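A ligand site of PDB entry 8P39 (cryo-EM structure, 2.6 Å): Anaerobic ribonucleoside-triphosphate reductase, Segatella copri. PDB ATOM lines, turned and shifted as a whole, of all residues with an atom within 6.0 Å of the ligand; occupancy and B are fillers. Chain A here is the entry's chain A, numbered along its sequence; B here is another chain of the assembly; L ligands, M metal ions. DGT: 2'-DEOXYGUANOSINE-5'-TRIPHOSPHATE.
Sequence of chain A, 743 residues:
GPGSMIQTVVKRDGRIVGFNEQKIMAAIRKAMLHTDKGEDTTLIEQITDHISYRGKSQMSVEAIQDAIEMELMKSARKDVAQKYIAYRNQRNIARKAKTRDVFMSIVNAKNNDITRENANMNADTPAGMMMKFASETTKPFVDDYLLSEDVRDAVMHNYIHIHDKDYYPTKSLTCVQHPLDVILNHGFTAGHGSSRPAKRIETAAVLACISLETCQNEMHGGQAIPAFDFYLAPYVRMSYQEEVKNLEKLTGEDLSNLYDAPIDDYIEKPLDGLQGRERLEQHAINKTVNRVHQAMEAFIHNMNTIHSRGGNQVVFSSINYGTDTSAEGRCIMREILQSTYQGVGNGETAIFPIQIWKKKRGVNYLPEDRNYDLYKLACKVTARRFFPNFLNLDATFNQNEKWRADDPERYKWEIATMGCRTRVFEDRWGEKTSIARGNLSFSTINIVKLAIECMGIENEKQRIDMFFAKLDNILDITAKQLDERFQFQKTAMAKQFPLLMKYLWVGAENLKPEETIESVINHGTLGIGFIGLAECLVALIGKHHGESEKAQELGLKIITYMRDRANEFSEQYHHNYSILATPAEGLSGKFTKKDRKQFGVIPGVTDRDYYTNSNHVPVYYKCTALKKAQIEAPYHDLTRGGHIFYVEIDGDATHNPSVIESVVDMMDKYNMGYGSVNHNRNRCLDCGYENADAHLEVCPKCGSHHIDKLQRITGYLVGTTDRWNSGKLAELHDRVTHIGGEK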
ATOM      1  N   SER A 194       0.305  23.508  -3.215  1.00  0.00           N
ATOM      2  CA  SER A 194       1.398  23.750  -4.146  1.00  0.00           C
ATOM      3  C   SER A 194       2.119  22.440  -4.449  1.00  0.00           C
ATOM      4  O   SER A 194       2.090  21.496  -3.662  1.00  0.00           O
ATOM      5  CB  SER A 194       2.388  24.773  -3.579  1.00  0.00           C
ATOM      6  OG  SER A 194       3.410  25.054  -4.513  1.00  0.00           O
ATOM      7  N   SER A 195       2.778  22.401  -5.610  1.00  0.00           N
ATOM      8  CA  SER A 195       3.510  21.228  -6.047  1.00  0.00           C
ATOM      9  C   SER A 195       4.755  21.661  -6.807  1.00  0.00           C
ATOM     10  O   SER A 195       4.884  22.811  -7.241  1.00  0.00           O
ATOM     11  CB  SER A 195       2.647  20.314  -6.930  1.00  0.00           C
ATOM     12  OG  SER A 195       1.536  19.819  -6.206  1.00  0.00           O
ATOM     13  N   ARG A 196       5.691  20.725  -6.956  1.00  0.00           N
ATOM     14  CA  ARG A 196       6.956  20.942  -7.637  1.00  0.00           C
ATOM     15  C   ARG A 196       6.921  20.345  -9.044  1.00  0.00           C
ATOM     16  O   ARG A 196       6.085  19.499  -9.346  1.00  0.00           O
ATOM     17  CB  ARG A 196       8.103  20.307  -6.841  1.00  0.00           C
ATOM     18  CG  ARG A 196       8.357  20.966  -5.493  1.00  0.00           C
ATOM     19  CD  ARG A 196       9.739  20.614  -4.965  1.00  0.00           C
ATOM     20  NE  ARG A 196       9.936  21.097  -3.602  1.00  0.00           N
ATOM     21  CZ  ARG A 196       9.793  20.349  -2.525  1.00  0.00           C
ATOM     22  NH1 ARG A 196       9.468  19.067  -2.601  1.00  0.00           N
ATOM     23  NH2 ARG A 196       9.977  20.894  -1.323  1.00  0.00           N
ATOM     24  N   PRO A 197       7.815  20.794  -9.927  1.00  0.00           N
ATOM     25  CA  PRO A 197       7.878  20.215 -11.272  1.00  0.00           C
ATOM     26  C   PRO A 197       8.158  18.713 -11.221  1.00  0.00           C
ATOM     27  O   PRO A 197       8.936  18.239 -10.391  1.00  0.00           O
ATOM     28  CB  PRO A 197       9.024  20.974 -11.938  1.00  0.00           C
ATOM     29  CG  PRO A 197       9.063  22.281 -11.229  1.00  0.00           C
ATOM     30  CD  PRO A 197       8.691  21.973  -9.804  1.00  0.00           C
ATOM     31  N   ALA A 198       7.519  17.983 -12.130  1.00  0.00           N
ATOM     32  CA  ALA A 198       7.658  16.532 -12.153  1.00  0.00           C
ATOM     33  C   ALA A 198       9.025  16.128 -12.682  1.00  0.00           C
ATOM     34  O   ALA A 198       9.592  16.775 -13.565  1.00  0.00           O
ATOM     35  CB  ALA A 198       6.562  15.908 -13.014  1.00  0.00           C
ATOM     36  N   LYS A 199       9.564  15.040 -12.121  1.00  0.00           N
ATOM     37  CA  LYS A 199      10.837  14.485 -12.570  1.00  0.00           C
ATOM     38  C   LYS A 199      10.776  12.969 -12.702  1.00  0.00           C
ATOM     39  O   LYS A 199      11.825  12.311 -12.654  1.00  0.00           O
ATOM     40  CB  LYS A 199      11.960  14.882 -11.610  1.00  0.00           C
ATOM     41  CG  LYS A 199      12.111  16.379 -11.399  1.00  0.00           C
ATOM     42  CD  LYS A 199      13.277  16.697 -10.466  1.00  0.00           C
ATOM     43  CE  LYS A 199      13.353  18.189 -10.160  1.00  0.00           C
ATOM     44  NZ  LYS A 199      13.519  19.003 -11.394  1.00  0.00           N
ATOM     45  N   ARG A 200       9.588  12.409 -12.847  1.00  0.00           N
ATOM     46  CA  ARG A 200       9.400  10.967 -12.925  1.00  0.00           C
ATOM     47  C   ARG A 200       8.064  10.692 -13.598  1.00  0.00           C
ATOM     48  O   ARG A 200       7.221  11.591 -13.717  1.00  0.00           O
ATOM     49  CB  ARG A 200       9.440  10.335 -11.528  1.00  0.00           C
ATOM     50  CG  ARG A 200       9.869   8.873 -11.499  1.00  0.00           C
ATOM     51  CD  ARG A 200       9.809   8.326 -10.086  1.00  0.00           C
ATOM     52  NE  ARG A 200      10.142   9.355  -9.103  1.00  0.00           N
ATOM     53  CZ  ARG A 200      11.371   9.675  -8.736  1.00  0.00           C
ATOM     54  NH1 ARG A 200      12.428   9.062  -9.251  1.00  0.00           N
ATOM     55  NH2 ARG A 200      11.551  10.638  -7.849  1.00  0.00           N
ATOM     56  N   GLU A 202       5.739   8.584 -12.484  1.00  0.00           N
ATOM     57  CA  GLU A 202       4.702   8.580 -11.464  1.00  0.00           C
ATOM     58  C   GLU A 202       4.272   9.997 -11.106  1.00  0.00           C
ATOM     59  O   GLU A 202       3.072  10.271 -10.958  1.00  0.00           O
ATOM     60  CB  GLU A 202       5.184   7.834 -10.223  1.00  0.00           C
ATOM     61  CG  GLU A 202       5.045   6.316 -10.299  1.00  0.00           C
ATOM     62  CD  GLU A 202       6.036   5.682 -11.250  1.00  0.00           C
ATOM     63  OE1 GLU A 202       7.067   6.326 -11.550  1.00  0.00           O
ATOM     64  OE2 GLU A 202       5.791   4.536 -11.689  1.00  0.00           O
ATOM     65  N   THR A 203       5.234  10.906 -10.970  1.00  0.00           N
ATOM     66  CA  THR A 203       4.904  12.267 -10.560  1.00  0.00           C
ATOM     67  C   THR A 203       4.236  13.038 -11.699  1.00  0.00           C
ATOM     68  O   THR A 203       3.385  13.903 -11.453  1.00  0.00           O
ATOM     69  CB  THR A 203       6.170  12.988 -10.103  1.00  0.00           C
ATOM     70  OG1 THR A 203       7.119  13.030 -11.174  1.00  0.00           O
ATOM     71  CG2 THR A 203       6.793  12.253  -8.920  1.00  0.00           C
ATOM     72  N   VAL A 206       0.408  11.806 -12.090  1.00  0.00           N
ATOM     73  CA  VAL A 206      -0.474  12.103 -10.967  1.00  0.00           C
ATOM     74  C   VAL A 206      -0.839  13.588 -10.949  1.00  0.00           C
ATOM     75  O   VAL A 206      -1.967  13.952 -10.601  1.00  0.00           O
ATOM     76  CB  VAL A 206       0.162  11.643  -9.641  1.00  0.00           C
ATOM     77  CG1 VAL A 206       1.388  12.469  -9.284  1.00  0.00           C
ATOM     78  CG2 VAL A 206      -0.864  11.680  -8.526  1.00  0.00           C
ATOM     79  N   LEU A 207       0.103  14.466 -11.317  1.00  0.00           N
ATOM     80  CA  LEU A 207      -0.190  15.897 -11.305  1.00  0.00           C
ATOM     81  C   LEU A 207      -1.149  16.273 -12.426  1.00  0.00           C
ATOM     82  O   LEU A 207      -1.855  17.288 -12.330  1.00  0.00           O
ATOM     83  CB  LEU A 207       1.103  16.697 -11.418  1.00  0.00           C
ATOM     84  CG  LEU A 207       1.898  16.881 -10.121  1.00  0.00           C
ATOM     85  CD1 LEU A 207       3.036  17.865 -10.324  1.00  0.00           C
ATOM     86  CD2 LEU A 207       0.982  17.338  -9.004  1.00  0.00           C
ATOM     87  N   ILE A 210      -4.716  16.212 -11.041  1.00  0.00           N
ATOM     88  CA  ILE A 210      -5.083  17.320 -10.169  1.00  0.00           C
ATOM     89  C   ILE A 210      -5.404  18.561 -10.986  1.00  0.00           C
ATOM     90  O   ILE A 210      -6.286  19.355 -10.621  1.00  0.00           O
ATOM     91  CB  ILE A 210      -3.969  17.573  -9.144  1.00  0.00           C
ATOM     92  CG1 ILE A 210      -3.570  16.267  -8.455  1.00  0.00           C
ATOM     93  CG2 ILE A 210      -4.423  18.584  -8.098  1.00  0.00           C
ATOM     94  CD1 ILE A 210      -2.385  16.405  -7.541  1.00  0.00           C
ATOM     95  N   ASN A 302      -7.222   7.336 -11.010  1.00  0.00           N
ATOM     96  CA  ASN A 302      -7.507   8.594 -10.338  1.00  0.00           C
ATOM     97  C   ASN A 302      -8.678   9.319 -10.968  1.00  0.00           C
ATOM     98  O   ASN A 302      -9.540   9.855 -10.262  1.00  0.00           O
ATOM     99  CB  ASN A 302      -6.254   9.488 -10.355  1.00  0.00           C
ATOM    100  CG  ASN A 302      -5.282   9.136  -9.249  1.00  0.00           C
ATOM    101  OD1 ASN A 302      -5.664   8.620  -8.213  1.00  0.00           O
ATOM    102  ND2 ASN A 302      -4.007   9.434  -9.482  1.00  0.00           N
ATOM    103  N   VAL B 206      -1.408   6.145  -1.242  1.00  0.00           N
ATOM    104  CA  VAL B 206      -2.391   6.844  -2.066  1.00  0.00           C
ATOM    105  C   VAL B 206      -3.817   6.379  -1.761  1.00  0.00           C
ATOM    106  O   VAL B 206      -4.766   7.152  -1.967  1.00  0.00           O
ATOM    107  CB  VAL B 206      -2.059   6.663  -3.558  1.00  0.00           C
ATOM    108  CG1 VAL B 206      -2.295   5.218  -3.996  1.00  0.00           C
ATOM    109  CG2 VAL B 206      -2.871   7.635  -4.412  1.00  0.00           C
ATOM    110  N   GLN B 294       9.219   8.672  -0.545  1.00  0.00           N
ATOM    111  CA  GLN B 294       8.363   9.246  -1.581  1.00  0.00           C
ATOM    112  C   GLN B 294       6.889   9.033  -1.272  1.00  0.00           C
ATOM    113  O   GLN B 294       6.057   9.914  -1.535  1.00  0.00           O
ATOM    114  CB  GLN B 294       8.722   8.658  -2.947  1.00  0.00           C
ATOM    115  CG  GLN B 294       9.955   9.282  -3.578  1.00  0.00           C
ATOM    116  CD  GLN B 294       9.710  10.700  -4.075  1.00  0.00           C
ATOM    117  OE1 GLN B 294       8.564  11.131  -4.216  1.00  0.00           O
ATOM    118  NE2 GLN B 294      10.784  11.427  -4.323  1.00  0.00           N
ATOM    119  N   GLU B 297       5.717  11.478   1.157  1.00  0.00           N
ATOM    120  CA  GLU B 297       5.666  12.779   0.487  1.00  0.00           C
ATOM    121  C   GLU B 297       4.370  12.941  -0.276  1.00  0.00           C
ATOM    122  O   GLU B 297       3.764  14.025  -0.290  1.00  0.00           O
ATOM    123  CB  GLU B 297       6.875  12.920  -0.440  1.00  0.00           C
ATOM    124  CG  GLU B 297       7.222  14.350  -0.810  1.00  0.00           C
ATOM    125  CD  GLU B 297       7.934  15.091   0.309  1.00  0.00           C
ATOM    126  OE1 GLU B 297       8.323  14.444   1.306  1.00  0.00           O
ATOM    127  OE2 GLU B 297       8.105  16.320   0.195  1.00  0.00           O
ATOM    128  N   ALA B 298       3.917  11.872  -0.934  1.00  0.00           N
ATOM    129  CA  ALA B 298       2.682  11.946  -1.726  1.00  0.00           C
ATOM    130  C   ALA B 298       1.457  12.098  -0.838  1.00  0.00           C
ATOM    131  O   ALA B 298       0.515  12.808  -1.189  1.00  0.00           O
ATOM    132  CB  ALA B 298       2.559  10.704  -2.604  1.00  0.00           C
ATOM    133  N   HIS B 301       1.107  15.789   0.381  1.00  0.00           N
ATOM    134  CA  HIS B 301       0.809  16.686  -0.730  1.00  0.00           C
ATOM    135  C   HIS B 301      -0.560  16.446  -1.340  1.00  0.00           C
ATOM    136  O   HIS B 301      -1.030  17.274  -2.122  1.00  0.00           O
ATOM    137  CB  HIS B 301       1.887  16.572  -1.802  1.00  0.00           C
ATOM    138  CG  HIS B 301       3.235  17.041  -1.365  1.00  0.00           C
ATOM    139  ND1 HIS B 301       3.982  16.393  -0.402  1.00  0.00           N
ATOM    140  CD2 HIS B 301       3.966  18.118  -1.754  1.00  0.00           C
ATOM    141  CE1 HIS B 301       5.119  17.038  -0.218  1.00  0.00           C
ATOM    142  NE2 HIS B 301       5.138  18.087  -1.028  1.00  0.00           N
ATOM    143  N   ASN B 302      -1.219  15.340  -1.000  1.00  0.00           N
ATOM    144  CA  ASN B 302      -2.566  15.058  -1.485  1.00  0.00           C
ATOM    145  C   ASN B 302      -3.629  15.379  -0.446  1.00  0.00           C
ATOM    146  O   ASN B 302      -4.809  15.079  -0.671  1.00  0.00           O
ATOM    147  CB  ASN B 302      -2.669  13.598  -1.915  1.00  0.00           C
ATOM    148  CG  ASN B 302      -3.799  13.351  -2.906  1.00  0.00           C
ATOM    149  OD1 ASN B 302      -4.248  14.276  -3.583  1.00  0.00           O
ATOM    150  ND2 ASN B 302      -4.263  12.113  -2.983  1.00  0.00           N
ATOM    151  N   MET B 303      -3.249  15.971   0.684  1.00  0.00           N
ATOM    152  CA  MET B 303      -4.193  16.397   1.708  1.00  0.00           C
ATOM    153  C   MET B 303      -4.325  17.909   1.803  1.00  0.00           C
ATOM    154  O   MET B 303      -5.420  18.421   2.062  1.00  0.00           O
ATOM    155  CB  MET B 303      -3.792  15.847   3.079  1.00  0.00           C
ATOM    156  CG  MET B 303      -3.779  14.327   3.150  1.00  0.00           C
ATOM    157  SD  MET B 303      -5.281  13.570   2.525  1.00  0.00           S
ATOM    158  CE  MET B 303      -6.499  14.267   3.632  1.00  0.00           C
ATOM    159  N   THR B 305      -3.588  19.872  -0.849  1.00  0.00           N
ATOM    160  CA  THR B 305      -4.068  20.281  -2.165  1.00  0.00           C
ATOM    161  C   THR B 305      -5.591  20.149  -2.260  1.00  0.00           C
ATOM    162  O   THR B 305      -6.256  21.043  -2.801  1.00  0.00           O
ATOM    163  CB  THR B 305      -3.388  19.460  -3.249  1.00  0.00           C
ATOM    164  OG1 THR B 305      -1.970  19.656  -3.185  1.00  0.00           O
ATOM    165  CG2 THR B 305      -3.887  19.865  -4.622  1.00  0.00           C
ATOM    166  N   GLN B 342       9.522  18.761   6.260  1.00  0.00           N
ATOM    167  CA  GLN B 342      10.032  19.329   5.018  1.00  0.00           C
ATOM    168  C   GLN B 342       9.033  20.285   4.386  1.00  0.00           C
ATOM    169  O   GLN B 342       9.377  21.413   4.028  1.00  0.00           O
ATOM    170  CB  GLN B 342      10.416  18.210   4.041  1.00  0.00           C
ATOM    171  CG  GLN B 342      11.242  18.672   2.861  1.00  0.00           C
ATOM    172  CD  GLN B 342      12.131  17.568   2.303  1.00  0.00           C
ATOM    173  OE1 GLN B 342      12.580  16.692   3.035  1.00  0.00           O
ATOM    174  NE2 GLN B 342      12.368  17.607   1.002  1.00  0.00           N
ATOM    175  N   VAL B 344       5.126  21.080   2.056  1.00  0.00           N
ATOM    176  CA  VAL B 344       4.463  20.941   0.769  1.00  0.00           C
ATOM    177  C   VAL B 344       4.935  22.043  -0.162  1.00  0.00           C
ATOM    178  O   VAL B 344       5.194  23.172   0.287  1.00  0.00           O
ATOM    179  CB  VAL B 344       2.924  20.976   0.931  1.00  0.00           C
ATOM    180  CG1 VAL B 344       2.226  20.823  -0.398  1.00  0.00           C
ATOM    181  CG2 VAL B 344       2.475  19.890   1.886  1.00  0.00           C
ATOM    182  N   GLY B 345       5.074  21.719  -1.444  1.00  0.00           N
ATOM    183  CA  GLY B 345       5.446  22.738  -2.417  1.00  0.00           C
ATOM    184  C   GLY B 345       6.813  23.307  -2.151  1.00  0.00           C
ATOM    185  O   GLY B 345       7.790  22.579  -1.937  1.00  0.00           O
HETATM  186  PG  DGT L   1      13.561  15.861  -5.513  1.00  0.00           P
HETATM  187  O1G DGT L   1      13.265  14.521  -6.140  1.00  0.00           O
HETATM  188  O2G DGT L   1      13.232  15.893  -4.041  1.00  0.00           O
HETATM  189  O3G DGT L   1      14.953  16.346  -5.814  1.00  0.00           O
HETATM  190  O3B DGT L   1      12.557  16.918  -6.221  1.00  0.00           O
HETATM  191  PB  DGT L   1      10.967  17.060  -6.271  1.00  0.00           P
HETATM  192  O1B DGT L   1      10.473  17.319  -4.884  1.00  0.00           O
HETATM  193  O2B DGT L   1      10.596  17.989  -7.373  1.00  0.00           O
HETATM  194  O3A DGT L   1      10.542  15.565  -6.677  1.00  0.00           O
HETATM  195  PA  DGT L   1       9.213  14.949  -7.333  1.00  0.00           P
HETATM  196  O1A DGT L   1       9.246  15.204  -8.802  1.00  0.00           O
HETATM  197  O2A DGT L   1       9.048  13.550  -6.847  1.00  0.00           O
HETATM  198  O5' DGT L   1       8.091  15.880  -6.678  1.00  0.00           O
HETATM  199  C5' DGT L   1       6.700  15.590  -6.969  1.00  0.00           C
HETATM  200  C4' DGT L   1       5.829  16.659  -6.368  1.00  0.00           C
HETATM  201  O4' DGT L   1       4.450  16.268  -6.514  1.00  0.00           O
HETATM  202  C3' DGT L   1       6.035  16.862  -4.875  1.00  0.00           C
HETATM  203  O3' DGT L   1       5.584  18.164  -4.507  1.00  0.00           O
HETATM  204  C2' DGT L   1       5.091  15.794  -4.325  1.00  0.00           C
HETATM  205  C1' DGT L   1       3.899  16.016  -5.228  1.00  0.00           C
HETATM  206  N9  DGT L   1       3.005  14.863  -5.332  1.00  0.00           N
HETATM  207  C8  DGT L   1       3.351  13.568  -5.631  1.00  0.00           C
HETATM  208  N7  DGT L   1       2.337  12.751  -5.658  1.00  0.00           N
HETATM  209  C5  DGT L   1       1.244  13.554  -5.359  1.00  0.00           C
HETATM  210  C6  DGT L   1      -0.130  13.226  -5.237  1.00  0.00           C
HETATM  211  O6  DGT L   1      -0.663  12.117  -5.382  1.00  0.00           O
HETATM  212  N1  DGT L   1      -0.895  14.341  -4.919  1.00  0.00           N
HETATM  213  C2  DGT L   1      -0.416  15.609  -4.736  1.00  0.00           C
HETATM  214  N2  DGT L   1      -1.315  16.561  -4.432  1.00  0.00           N
HETATM  215  N3  DGT L   1       0.874  15.930  -4.841  1.00  0.00           N
HETATM  216  C4  DGT L   1       1.643  14.860  -5.156  1.00  0.00           C
HETATM  217 MG    MG M   1      11.859  13.132  -4.044  1.00  0.00          MG
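The guanidinium group (NH2) of Arg 200 lies within salt-bridge range of an oxygen (O2A) of the ligand (3.97 Å).
O of His 301 of chain B is in hydrogen-bond range of N2 of the ligand, 2.4 Å away.
O1A of the ligand is in hydrogen-bond range of N of Lys 199, 3.3 Å away.
A nitrogen (N2) of the ligand sits at hydrogen-bond distance from the side-chain hydroxyl (OG1) of Thr 305 of chain B, at 3.4 Å.
The guanidinium group of Arg 196 lies within salt-bridge range of an oxygen (O1B) of the ligand.
OG1 of Thr 203 lies within hydrogen-bond range of O of Arg 200, at 2.9 Å.
N of Lys 199 sits at hydrogen-bond distance from OG1 of Thr 203.
The guanidinium group (NH2) of Arg 196 is in hydrogen-bond range of the backbone carbonyl oxygen (O) of Gly 345 of chain B, 2.8 Å away.
O of His 301 of chain B lies within hydrogen-bond range of OG1 of Thr 305 of chain B.
The backbone carbonyl oxygen of Pro 197 lies close to an oxygen (O1A) of the ligand (3.4 Å).
Merely in contact with the ligand: Val 206 of chain A (3.2 Å), Ile 210 (3.3 Å), Thr 203 (3.3 Å), Asn 302 of chain B (3.5 Å), Gln 294 of chain B (3.6 Å), Ala 298 of chain B (3.7 Å) and Ala 198 (3.9 Å).
Hydrophobic or aromatic side chains within 4 Å of the ligand: Val 206 of chain A, Ile 210, Ala 298 of chain B and His 301 of chain B.
The nearest printed residue that does not touch the ligand is Ser 195 (4.01 Å).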
